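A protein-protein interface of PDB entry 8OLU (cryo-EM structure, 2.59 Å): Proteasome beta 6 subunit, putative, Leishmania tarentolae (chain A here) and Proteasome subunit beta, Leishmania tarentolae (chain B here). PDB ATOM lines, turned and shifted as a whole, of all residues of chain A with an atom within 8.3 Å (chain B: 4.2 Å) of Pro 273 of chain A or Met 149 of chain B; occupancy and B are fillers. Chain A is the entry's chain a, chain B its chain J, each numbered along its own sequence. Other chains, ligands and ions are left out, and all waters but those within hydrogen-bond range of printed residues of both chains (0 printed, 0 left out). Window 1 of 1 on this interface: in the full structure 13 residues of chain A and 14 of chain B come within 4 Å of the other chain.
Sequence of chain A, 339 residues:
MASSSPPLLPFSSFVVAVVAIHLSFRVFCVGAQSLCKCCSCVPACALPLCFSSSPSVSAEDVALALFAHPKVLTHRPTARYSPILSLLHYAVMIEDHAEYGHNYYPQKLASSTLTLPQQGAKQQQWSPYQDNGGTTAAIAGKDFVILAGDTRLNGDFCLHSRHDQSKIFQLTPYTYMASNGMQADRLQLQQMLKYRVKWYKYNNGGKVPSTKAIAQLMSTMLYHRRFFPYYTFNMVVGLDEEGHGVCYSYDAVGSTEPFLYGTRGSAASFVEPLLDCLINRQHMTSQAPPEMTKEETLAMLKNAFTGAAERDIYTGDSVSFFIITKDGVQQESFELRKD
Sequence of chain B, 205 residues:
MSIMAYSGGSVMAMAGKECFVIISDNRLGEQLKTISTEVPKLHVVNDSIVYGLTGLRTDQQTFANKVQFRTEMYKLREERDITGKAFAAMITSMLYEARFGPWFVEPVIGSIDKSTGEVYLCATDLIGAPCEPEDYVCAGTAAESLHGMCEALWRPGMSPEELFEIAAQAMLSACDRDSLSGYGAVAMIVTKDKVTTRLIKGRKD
Phe 270 of chain A touches Gly 148 of chain B (O to CA, 3.6 Å). Pro 273 of chain A touches Ser 145 of chain B. Pro 273 of chain A touches Ser 173 of chain B. Ala 152 of chain B touches Leu 274 of chain A. Cys 277 of chain A touches Met 149 of chain B (CB to CE, 3.9 Å). OE1 of Gln 169 of chain B touches CE of Met 284 of chain A (3.7 Å). Gly 307 of chain A touches Glu 151 of chain B.
Printed residues of chain B within 4 Å of Phe 270 of chain A: Gly 148 (3.6 Å). Of the printed residues of chain B, Pro 273 of chain A touches Ser 145, Met 149 and Ser 173. Of the printed residues of chain B, Cys 277 of chain A touches Met 149 and Ser 173. Of the printed residues of chain B, Met 284 of chain A touches Gln 169. Printed residues of chain B within 4 Å of Gly 307 of chain A: Glu 151. Printed residues of chain B within 4 Å of Arg 311 of chain A: Glu 151. Gly 148 of chain B touches just one residue of chain A: Phe 270 (3.6 Å). Printed residues of chain A within 4 Å of Met 149 of chain B: Pro 273, Leu 274 and Cys 277.
O of Ser 269 of chain A lies within hydrogen-bond range of OG of Ser 145 of chain B (2.9 Å). The side-chain sulfur of Met 149 of chain B lies close to the backbone NH of Leu 274 of chain A, 3.6 Å away. OE2 of Glu 151 of chain B is in salt-bridge range of NE of Arg 311 of chain A (2.6 Å). SG of Cys 277 of chain A sits close to OG of Ser 173 of chain B (3.5 Å). The side-chain sulfur (SD) of Met 149 of chain B lies close to the backbone carbonyl oxygen (O) of Pro 273 of chain A (3.3 Å).
O of Gln 169 of chain B sits at hydrogen-bond distance from OG of Ser 173 of chain B (2.6 Å). The side-chain sulfur (SD) of Met 284 of chain A lies close to the guanidinium group (NE) of Arg 281 of chain A, at 3.4 Å.
Printed residues of chain A that touch a printed residue of chain B: Ser 269, Phe 270, Pro 273, Leu 274, Cys 277, Met 284, Gly 307 and Arg 311. Hydrophobic or aromatic side chains of chain A within 4 Å of the printed part of chain B: Phe 270, Pro 273, Leu 274 and Met 284. Of the 12 printed residues of chain B, 7 touch a printed residue of chain A. Among the printed residues, 12 pairs touch across the chains.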
ATOM      1  N   TYR A 261      -6.977   3.268  16.668  1.00  0.00           N
ATOM      2  CA  TYR A 261      -8.102   3.951  17.238  1.00  0.00           C
ATOM      3  C   TYR A 261      -9.156   4.267  16.190  1.00  0.00           C
ATOM      4  O   TYR A 261      -9.339   3.546  15.184  1.00  0.00           O
ATOM      5  CB  TYR A 261      -7.620   5.140  18.023  1.00  0.00           C
ATOM      6  CG  TYR A 261      -6.876   6.140  17.211  1.00  0.00           C
ATOM      7  CD1 TYR A 261      -7.533   7.099  16.476  1.00  0.00           C
ATOM      8  CD2 TYR A 261      -5.495   6.161  17.253  1.00  0.00           C
ATOM      9  CE1 TYR A 261      -6.819   8.086  15.817  1.00  0.00           C
ATOM     10  CE2 TYR A 261      -4.771   7.105  16.560  1.00  0.00           C
ATOM     11  CZ  TYR A 261      -5.434   8.083  15.852  1.00  0.00           C
ATOM     12  OH  TYR A 261      -4.659   8.992  15.163  1.00  0.00           O
ATOM     13  N   THR A 263     -13.263   6.428  15.745  1.00  0.00           N
ATOM     14  CA  THR A 263     -14.430   7.109  16.239  1.00  0.00           C
ATOM     15  C   THR A 263     -15.325   7.414  15.052  1.00  0.00           C
ATOM     16  O   THR A 263     -14.909   8.029  14.088  1.00  0.00           O
ATOM     17  CB  THR A 263     -13.985   8.340  17.038  1.00  0.00           C
ATOM     18  OG1 THR A 263     -15.060   9.001  17.708  1.00  0.00           O
ATOM     19  CG2 THR A 263     -13.309   9.296  16.106  1.00  0.00           C
ATOM     20  N   ALA A 267     -19.887  13.120  16.966  1.00  0.00           N
ATOM     21  CA  ALA A 267     -18.733  13.790  17.554  1.00  0.00           C
ATOM     22  C   ALA A 267     -17.421  13.333  16.943  1.00  0.00           C
ATOM     23  O   ALA A 267     -16.376  13.656  17.434  1.00  0.00           O
ATOM     24  CB  ALA A 267     -18.677  13.544  19.023  1.00  0.00           C
ATOM     25  N   ALA A 268     -17.472  12.533  15.902  1.00  0.00           N
ATOM     26  CA  ALA A 268     -16.269  11.899  15.422  1.00  0.00           C
ATOM     27  C   ALA A 268     -15.262  12.940  15.052  1.00  0.00           C
ATOM     28  O   ALA A 268     -14.099  12.806  15.350  1.00  0.00           O
ATOM     29  CB  ALA A 268     -16.582  11.100  14.197  1.00  0.00           C
ATOM     30  N   SER A 269     -15.745  13.969  14.389  1.00  0.00           N
ATOM     31  CA  SER A 269     -14.879  14.937  13.763  1.00  0.00           C
ATOM     32  C   SER A 269     -14.303  15.859  14.802  1.00  0.00           C
ATOM     33  O   SER A 269     -13.630  16.771  14.381  1.00  0.00           O
ATOM     34  CB  SER A 269     -15.616  15.711  12.684  1.00  0.00           C
ATOM     35  OG  SER A 269     -16.581  16.593  13.248  1.00  0.00           O
ATOM     36  N   PHE A 270     -14.651  15.683  16.080  1.00  0.00           N
ATOM     37  CA  PHE A 270     -14.045  16.403  17.184  1.00  0.00           C
ATOM     38  C   PHE A 270     -13.030  15.560  17.907  1.00  0.00           C
ATOM     39  O   PHE A 270     -11.999  16.053  18.372  1.00  0.00           O
ATOM     40  CB  PHE A 270     -14.879  16.492  18.459  1.00  0.00           C
ATOM     41  CG  PHE A 270     -16.048  17.386  18.344  1.00  0.00           C
ATOM     42  CD1 PHE A 270     -16.224  18.184  17.239  1.00  0.00           C
ATOM     43  CD2 PHE A 270     -16.973  17.418  19.343  1.00  0.00           C
ATOM     44  CE1 PHE A 270     -17.310  19.033  17.122  1.00  0.00           C
ATOM     45  CE2 PHE A 270     -18.089  18.228  19.200  1.00  0.00           C
ATOM     46  CZ  PHE A 270     -18.255  19.042  18.094  1.00  0.00           C
ATOM     47  N   VAL A 271     -13.437  14.324  18.129  1.00  0.00           N
ATOM     48  CA  VAL A 271     -12.692  13.424  18.950  1.00  0.00           C
ATOM     49  C   VAL A 271     -11.488  12.954  18.153  1.00  0.00           C
ATOM     50  O   VAL A 271     -10.379  12.967  18.671  1.00  0.00           O
ATOM     51  CB  VAL A 271     -13.649  12.300  19.348  1.00  0.00           C
ATOM     52  CG1 VAL A 271     -12.941  11.061  19.873  1.00  0.00           C
ATOM     53  CG2 VAL A 271     -14.677  12.842  20.329  1.00  0.00           C
ATOM     54  N   GLU A 272     -11.711  12.598  16.885  1.00  0.00           N
ATOM     55  CA  GLU A 272     -10.719  11.913  16.080  1.00  0.00           C
ATOM     56  C   GLU A 272      -9.483  12.773  16.036  1.00  0.00           C
ATOM     57  O   GLU A 272      -8.411  12.268  16.288  1.00  0.00           O
ATOM     58  CB  GLU A 272     -11.229  11.562  14.688  1.00  0.00           C
ATOM     59  CG  GLU A 272     -10.521  10.395  13.967  1.00  0.00           C
ATOM     60  CD  GLU A 272     -11.357   9.555  12.965  1.00  0.00           C
ATOM     61  OE1 GLU A 272     -12.307  10.113  12.300  1.00  0.00           O
ATOM     62  OE2 GLU A 272     -11.068   8.314  12.816  1.00  0.00           O
ATOM     63  N   PRO A 273      -9.534  14.078  15.775  1.00  0.00           N
ATOM     64  CA  PRO A 273      -8.329  14.872  15.774  1.00  0.00           C
ATOM     65  C   PRO A 273      -7.666  14.981  17.101  1.00  0.00           C
ATOM     66  O   PRO A 273      -6.491  15.292  17.120  1.00  0.00           O
ATOM     67  CB  PRO A 273      -8.680  16.304  15.411  1.00  0.00           C
ATOM     68  CG  PRO A 273     -10.160  16.289  15.192  1.00  0.00           C
ATOM     69  CD  PRO A 273     -10.635  14.830  15.199  1.00  0.00           C
ATOM     70  N   LEU A 274      -8.425  14.857  18.172  1.00  0.00           N
ATOM     71  CA  LEU A 274      -7.801  14.952  19.475  1.00  0.00           C
ATOM     72  C   LEU A 274      -7.020  13.660  19.752  1.00  0.00           C
ATOM     73  O   LEU A 274      -5.919  13.672  20.297  1.00  0.00           O
ATOM     74  CB  LEU A 274      -8.901  15.176  20.515  1.00  0.00           C
ATOM     75  CG  LEU A 274      -8.400  15.036  21.949  1.00  0.00           C
ATOM     76  CD1 LEU A 274      -7.469  16.194  22.295  1.00  0.00           C
ATOM     77  CD2 LEU A 274      -9.537  14.904  22.949  1.00  0.00           C
ATOM     78  N   LEU A 275      -7.625  12.514  19.448  1.00  0.00           N
ATOM     79  CA  LEU A 275      -6.901  11.276  19.624  1.00  0.00           C
ATOM     80  C   LEU A 275      -5.657  11.299  18.748  1.00  0.00           C
ATOM     81  O   LEU A 275      -4.596  10.909  19.200  1.00  0.00           O
ATOM     82  CB  LEU A 275      -7.804  10.127  19.232  1.00  0.00           C
ATOM     83  CG  LEU A 275      -9.003   9.919  20.142  1.00  0.00           C
ATOM     84  CD1 LEU A 275      -9.721   8.612  19.771  1.00  0.00           C
ATOM     85  CD2 LEU A 275      -8.578   9.890  21.598  1.00  0.00           C
ATOM     86  N   ASP A 276      -5.771  11.794  17.509  1.00  0.00           N
ATOM     87  CA  ASP A 276      -4.614  11.924  16.644  1.00  0.00           C
ATOM     88  C   ASP A 276      -3.551  12.610  17.457  1.00  0.00           C
ATOM     89  O   ASP A 276      -2.509  12.050  17.678  1.00  0.00           O
ATOM     90  CB  ASP A 276      -4.854  12.737  15.371  1.00  0.00           C
ATOM     91  CG  ASP A 276      -5.725  12.075  14.303  1.00  0.00           C
ATOM     92  OD1 ASP A 276      -5.961  10.845  14.431  1.00  0.00           O
ATOM     93  OD2 ASP A 276      -6.186  12.805  13.352  1.00  0.00           O
ATOM     94  N   CYS A 277      -3.882  13.752  18.020  1.00  0.00           N
ATOM     95  CA  CYS A 277      -2.905  14.578  18.707  1.00  0.00           C
ATOM     96  C   CYS A 277      -2.261  13.879  19.917  1.00  0.00           C
ATOM     97  O   CYS A 277      -1.121  14.165  20.215  1.00  0.00           O
ATOM     98  CB  CYS A 277      -3.592  15.880  19.091  1.00  0.00           C
ATOM     99  SG  CYS A 277      -2.617  17.086  20.027  1.00  0.00           S
ATOM    100  N   LEU A 278      -2.941  13.028  20.669  1.00  0.00           N
ATOM    101  CA  LEU A 278      -2.414  12.658  21.982  1.00  0.00           C
ATOM    102  C   LEU A 278      -1.765  11.288  21.932  1.00  0.00           C
ATOM    103  O   LEU A 278      -0.899  10.981  22.747  1.00  0.00           O
ATOM    104  CB  LEU A 278      -3.530  12.665  23.034  1.00  0.00           C
ATOM    105  CG  LEU A 278      -4.307  13.983  23.102  1.00  0.00           C
ATOM    106  CD1 LEU A 278      -5.409  13.944  24.157  1.00  0.00           C
ATOM    107  CD2 LEU A 278      -3.337  15.139  23.344  1.00  0.00           C
ATOM    108  N   ILE A 279      -2.225  10.492  20.976  1.00  0.00           N
ATOM    109  CA  ILE A 279      -1.643   9.210  20.667  1.00  0.00           C
ATOM    110  C   ILE A 279      -0.427   9.361  19.768  1.00  0.00           C
ATOM    111  O   ILE A 279       0.625   8.864  20.148  1.00  0.00           O
ATOM    112  CB  ILE A 279      -2.728   8.349  20.042  1.00  0.00           C
ATOM    113  CG1 ILE A 279      -3.902   8.242  21.017  1.00  0.00           C
ATOM    114  CG2 ILE A 279      -2.154   7.007  19.623  1.00  0.00           C
ATOM    115  CD1 ILE A 279      -4.989   7.282  20.622  1.00  0.00           C
ATOM    116  N   ASN A 280      -0.557  10.029  18.606  1.00  0.00           N
ATOM    117  CA  ASN A 280       0.504  10.041  17.602  1.00  0.00           C
ATOM    118  C   ASN A 280       1.489  11.181  17.817  1.00  0.00           C
ATOM    119  O   ASN A 280       2.659  11.050  17.475  1.00  0.00           O
ATOM    120  CB  ASN A 280      -0.015  10.064  16.160  1.00  0.00           C
ATOM    121  CG  ASN A 280      -0.866   8.853  15.853  1.00  0.00           C
ATOM    122  OD1 ASN A 280      -1.863   8.936  15.132  1.00  0.00           O
ATOM    123  ND2 ASN A 280      -0.457   7.703  16.371  1.00  0.00           N
ATOM    124  N   ARG A 281       1.006  12.322  18.274  1.00  0.00           N
ATOM    125  CA  ARG A 281       1.860  13.447  18.642  1.00  0.00           C
ATOM    126  C   ARG A 281       2.803  13.905  17.522  1.00  0.00           C
ATOM    127  O   ARG A 281       3.900  14.381  17.809  1.00  0.00           O
ATOM    128  CB  ARG A 281       2.642  13.082  19.899  1.00  0.00           C
ATOM    129  CG  ARG A 281       1.805  12.306  20.903  1.00  0.00           C
ATOM    130  CD  ARG A 281       2.537  12.036  22.194  1.00  0.00           C
ATOM    131  NE  ARG A 281       3.012  13.241  22.864  1.00  0.00           N
ATOM    132  CZ  ARG A 281       2.447  13.771  23.948  1.00  0.00           C
ATOM    133  NH1 ARG A 281       1.154  13.594  24.197  1.00  0.00           N
ATOM    134  NH2 ARG A 281       3.190  14.523  24.745  1.00  0.00           N
ATOM    135  N   MET A 284       4.547  17.267  17.916  1.00  0.00           N
ATOM    136  CA  MET A 284       5.234  17.559  19.172  1.00  0.00           C
ATOM    137  C   MET A 284       6.715  17.152  19.099  1.00  0.00           C
ATOM    138  O   MET A 284       7.026  16.031  18.684  1.00  0.00           O
ATOM    139  CB  MET A 284       4.509  16.816  20.296  1.00  0.00           C
ATOM    140  CG  MET A 284       3.234  17.514  20.733  1.00  0.00           C
ATOM    141  SD  MET A 284       2.288  16.447  21.822  1.00  0.00           S
ATOM    142  CE  MET A 284       0.589  16.925  21.491  1.00  0.00           C
ATOM    143  N   ASN A 303     -11.952  11.904  28.766  1.00  0.00           N
ATOM    144  CA  ASN A 303     -11.733  13.319  28.611  1.00  0.00           C
ATOM    145  C   ASN A 303     -12.332  13.730  27.268  1.00  0.00           C
ATOM    146  O   ASN A 303     -12.808  14.859  27.107  1.00  0.00           O
ATOM    147  CB  ASN A 303     -10.270  13.703  28.750  1.00  0.00           C
ATOM    148  CG  ASN A 303     -10.076  15.192  28.522  1.00  0.00           C
ATOM    149  OD1 ASN A 303     -10.489  15.988  29.362  1.00  0.00           O
ATOM    150  ND2 ASN A 303      -9.488  15.604  27.399  1.00  0.00           N
ATOM    151  N   GLY A 307     -15.521  16.404  26.606  1.00  0.00           N
ATOM    152  CA  GLY A 307     -15.495  17.519  25.676  1.00  0.00           C
ATOM    153  C   GLY A 307     -16.492  17.365  24.537  1.00  0.00           C
ATOM    154  O   GLY A 307     -17.128  18.315  24.116  1.00  0.00           O
ATOM    155  N   ARG A 311     -20.094  19.898  23.277  1.00  0.00           N
ATOM    156  CA  ARG A 311     -20.046  20.707  22.074  1.00  0.00           C
ATOM    157  C   ARG A 311     -20.840  20.101  20.946  1.00  0.00           C
ATOM    158  O   ARG A 311     -21.274  20.808  20.083  1.00  0.00           O
ATOM    159  CB  ARG A 311     -18.621  20.902  21.597  1.00  0.00           C
ATOM    160  CG  ARG A 311     -17.823  21.715  22.604  1.00  0.00           C
ATOM    161  CD  ARG A 311     -17.734  23.150  22.206  1.00  0.00           C
ATOM    162  NE  ARG A 311     -17.220  23.905  23.324  1.00  0.00           N
ATOM    163  CZ  ARG A 311     -17.163  25.224  23.320  1.00  0.00           C
ATOM    164  NH1 ARG A 311     -17.862  25.910  22.421  1.00  0.00           N
ATOM    165  NH2 ARG A 311     -16.339  25.837  24.150  1.00  0.00           N
ATOM    166  N   SER B 145     -13.314  20.420  13.884  1.00  0.00           N
ATOM    167  CA  SER B 145     -12.200  19.784  14.556  1.00  0.00           C
ATOM    168  C   SER B 145     -11.513  20.751  15.485  1.00  0.00           C
ATOM    169  O   SER B 145     -10.848  20.389  16.434  1.00  0.00           O
ATOM    170  CB  SER B 145     -11.268  19.263  13.574  1.00  0.00           C
ATOM    171  OG  SER B 145     -11.936  18.411  12.637  1.00  0.00           O
ATOM    172  N   LEU B 146     -11.635  22.028  15.218  1.00  0.00           N
ATOM    173  CA  LEU B 146     -10.912  22.969  16.043  1.00  0.00           C
ATOM    174  C   LEU B 146     -11.580  23.174  17.410  1.00  0.00           C
ATOM    175  O   LEU B 146     -10.923  23.474  18.414  1.00  0.00           O
ATOM    176  CB  LEU B 146     -10.925  24.247  15.239  1.00  0.00           C
ATOM    177  CG  LEU B 146      -9.684  24.481  14.406  1.00  0.00           C
ATOM    178  CD1 LEU B 146      -9.850  25.794  13.639  1.00  0.00           C
ATOM    179  CD2 LEU B 146      -8.464  24.531  15.317  1.00  0.00           C
ATOM    180  N   HIS B 147     -12.915  23.085  17.392  1.00  0.00           N
ATOM    181  CA  HIS B 147     -13.747  23.040  18.576  1.00  0.00           C
ATOM    182  C   HIS B 147     -13.401  21.792  19.365  1.00  0.00           C
ATOM    183  O   HIS B 147     -13.232  21.831  20.572  1.00  0.00           O
ATOM    184  CB  HIS B 147     -15.235  23.021  18.176  1.00  0.00           C
ATOM    185  CG  HIS B 147     -15.795  24.364  17.880  1.00  0.00           C
ATOM    186  ND1 HIS B 147     -15.723  25.413  18.793  1.00  0.00           N
ATOM    187  CD2 HIS B 147     -16.361  24.821  16.716  1.00  0.00           C
ATOM    188  CE1 HIS B 147     -16.237  26.505  18.205  1.00  0.00           C
ATOM    189  NE2 HIS B 147     -16.645  26.155  16.906  1.00  0.00           N
ATOM    190  N   GLY B 148     -13.290  20.672  18.666  1.00  0.00           N
ATOM    191  CA  GLY B 148     -12.783  19.482  19.316  1.00  0.00           C
ATOM    192  C   GLY B 148     -11.569  19.798  20.167  1.00  0.00           C
ATOM    193  O   GLY B 148     -11.551  19.513  21.359  1.00  0.00           O
ATOM    194  N   MET B 149     -10.587  20.432  19.539  1.00  0.00           N
ATOM    195  CA  MET B 149      -9.271  20.434  20.115  1.00  0.00           C
ATOM    196  C   MET B 149      -9.237  21.493  21.177  1.00  0.00           C
ATOM    197  O   MET B 149      -8.613  21.317  22.197  1.00  0.00           O
ATOM    198  CB  MET B 149      -8.226  20.744  19.049  1.00  0.00           C
ATOM    199  CG  MET B 149      -8.241  19.685  17.921  1.00  0.00           C
ATOM    200  SD  MET B 149      -7.328  18.251  18.379  1.00  0.00           S
ATOM    201  CE  MET B 149      -5.955  18.953  19.316  1.00  0.00           C
ATOM    202  N   CYS B 150      -9.886  22.606  20.915  1.00  0.00           N
ATOM    203  CA  CYS B 150      -9.777  23.718  21.833  1.00  0.00           C
ATOM    204  C   CYS B 150     -10.535  23.373  23.113  1.00  0.00           C
ATOM    205  O   CYS B 150     -10.065  23.651  24.194  1.00  0.00           O
ATOM    206  CB  CYS B 150     -10.320  24.984  21.169  1.00  0.00           C
ATOM    207  SG  CYS B 150      -9.328  25.617  19.780  1.00  0.00           S
ATOM    208  N   GLU B 151     -11.684  22.713  22.986  1.00  0.00           N
ATOM    209  CA  GLU B 151     -12.411  22.224  24.150  1.00  0.00           C
ATOM    210  C   GLU B 151     -11.506  21.414  25.075  1.00  0.00           C
ATOM    211  O   GLU B 151     -11.468  21.627  26.283  1.00  0.00           O
ATOM    212  CB  GLU B 151     -13.578  21.309  23.744  1.00  0.00           C
ATOM    213  CG  GLU B 151     -14.562  21.041  24.875  1.00  0.00           C
ATOM    214  CD  GLU B 151     -14.990  22.257  25.709  1.00  0.00           C
ATOM    215  OE1 GLU B 151     -14.882  22.185  26.968  1.00  0.00           O
ATOM    216  OE2 GLU B 151     -15.439  23.292  25.110  1.00  0.00           O
ATOM    217  N   ALA B 152     -10.813  20.470  24.447  1.00  0.00           N
ATOM    218  CA  ALA B 152      -9.943  19.522  25.108  1.00  0.00           C
ATOM    219  C   ALA B 152      -8.733  20.164  25.761  1.00  0.00           C
ATOM    220  O   ALA B 152      -8.451  19.909  26.920  1.00  0.00           O
ATOM    221  CB  ALA B 152      -9.510  18.550  24.071  1.00  0.00           C
ATOM    222  N   LEU B 153      -8.081  21.060  25.034  1.00  0.00           N
ATOM    223  CA  LEU B 153      -6.768  21.532  25.414  1.00  0.00           C
ATOM    224  C   LEU B 153      -6.824  22.822  26.191  1.00  0.00           C
ATOM    225  O   LEU B 153      -5.950  23.044  27.023  1.00  0.00           O
ATOM    226  CB  LEU B 153      -5.960  21.769  24.146  1.00  0.00           C
ATOM    227  CG  LEU B 153      -5.692  20.522  23.314  1.00  0.00           C
ATOM    228  CD1 LEU B 153      -4.916  20.899  22.059  1.00  0.00           C
ATOM    229  CD2 LEU B 153      -4.935  19.489  24.122  1.00  0.00           C
ATOM    230  N   GLN B 169      -1.048  23.234  18.508  1.00  0.00           N
ATOM    231  CA  GLN B 169      -1.426  21.839  18.434  1.00  0.00           C
ATOM    232  C   GLN B 169      -2.848  21.668  17.937  1.00  0.00           C
ATOM    233  O   GLN B 169      -3.178  20.710  17.239  1.00  0.00           O
ATOM    234  CB  GLN B 169      -1.255  21.112  19.766  1.00  0.00           C
ATOM    235  CG  GLN B 169       0.216  21.009  20.170  1.00  0.00           C
ATOM    236  CD  GLN B 169       1.058  20.280  19.148  1.00  0.00           C
ATOM    237  OE1 GLN B 169       0.640  19.243  18.605  1.00  0.00           O
ATOM    238  NE2 GLN B 169       2.234  20.841  18.874  1.00  0.00           N
ATOM    239  N   ALA B 170      -3.691  22.590  18.327  1.00  0.00           N
ATOM    240  CA  ALA B 170      -5.092  22.488  17.949  1.00  0.00           C
ATOM    241  C   ALA B 170      -5.260  22.820  16.472  1.00  0.00           C
ATOM    242  O   ALA B 170      -5.902  22.058  15.737  1.00  0.00           O
ATOM    243  CB  ALA B 170      -5.918  23.393  18.841  1.00  0.00           C
ATOM    244  N   SER B 173      -3.598  19.851  14.568  1.00  0.00           N
ATOM    245  CA  SER B 173      -4.301  18.584  14.625  1.00  0.00           C
ATOM    246  C   SER B 173      -5.574  18.652  13.814  1.00  0.00           C
ATOM    247  O   SER B 173      -5.987  17.688  13.206  1.00  0.00           O
ATOM    248  CB  SER B 173      -4.543  18.176  16.036  1.00  0.00           C
ATOM    249  OG  SER B 173      -3.296  18.132  16.734  1.00  0.00           O
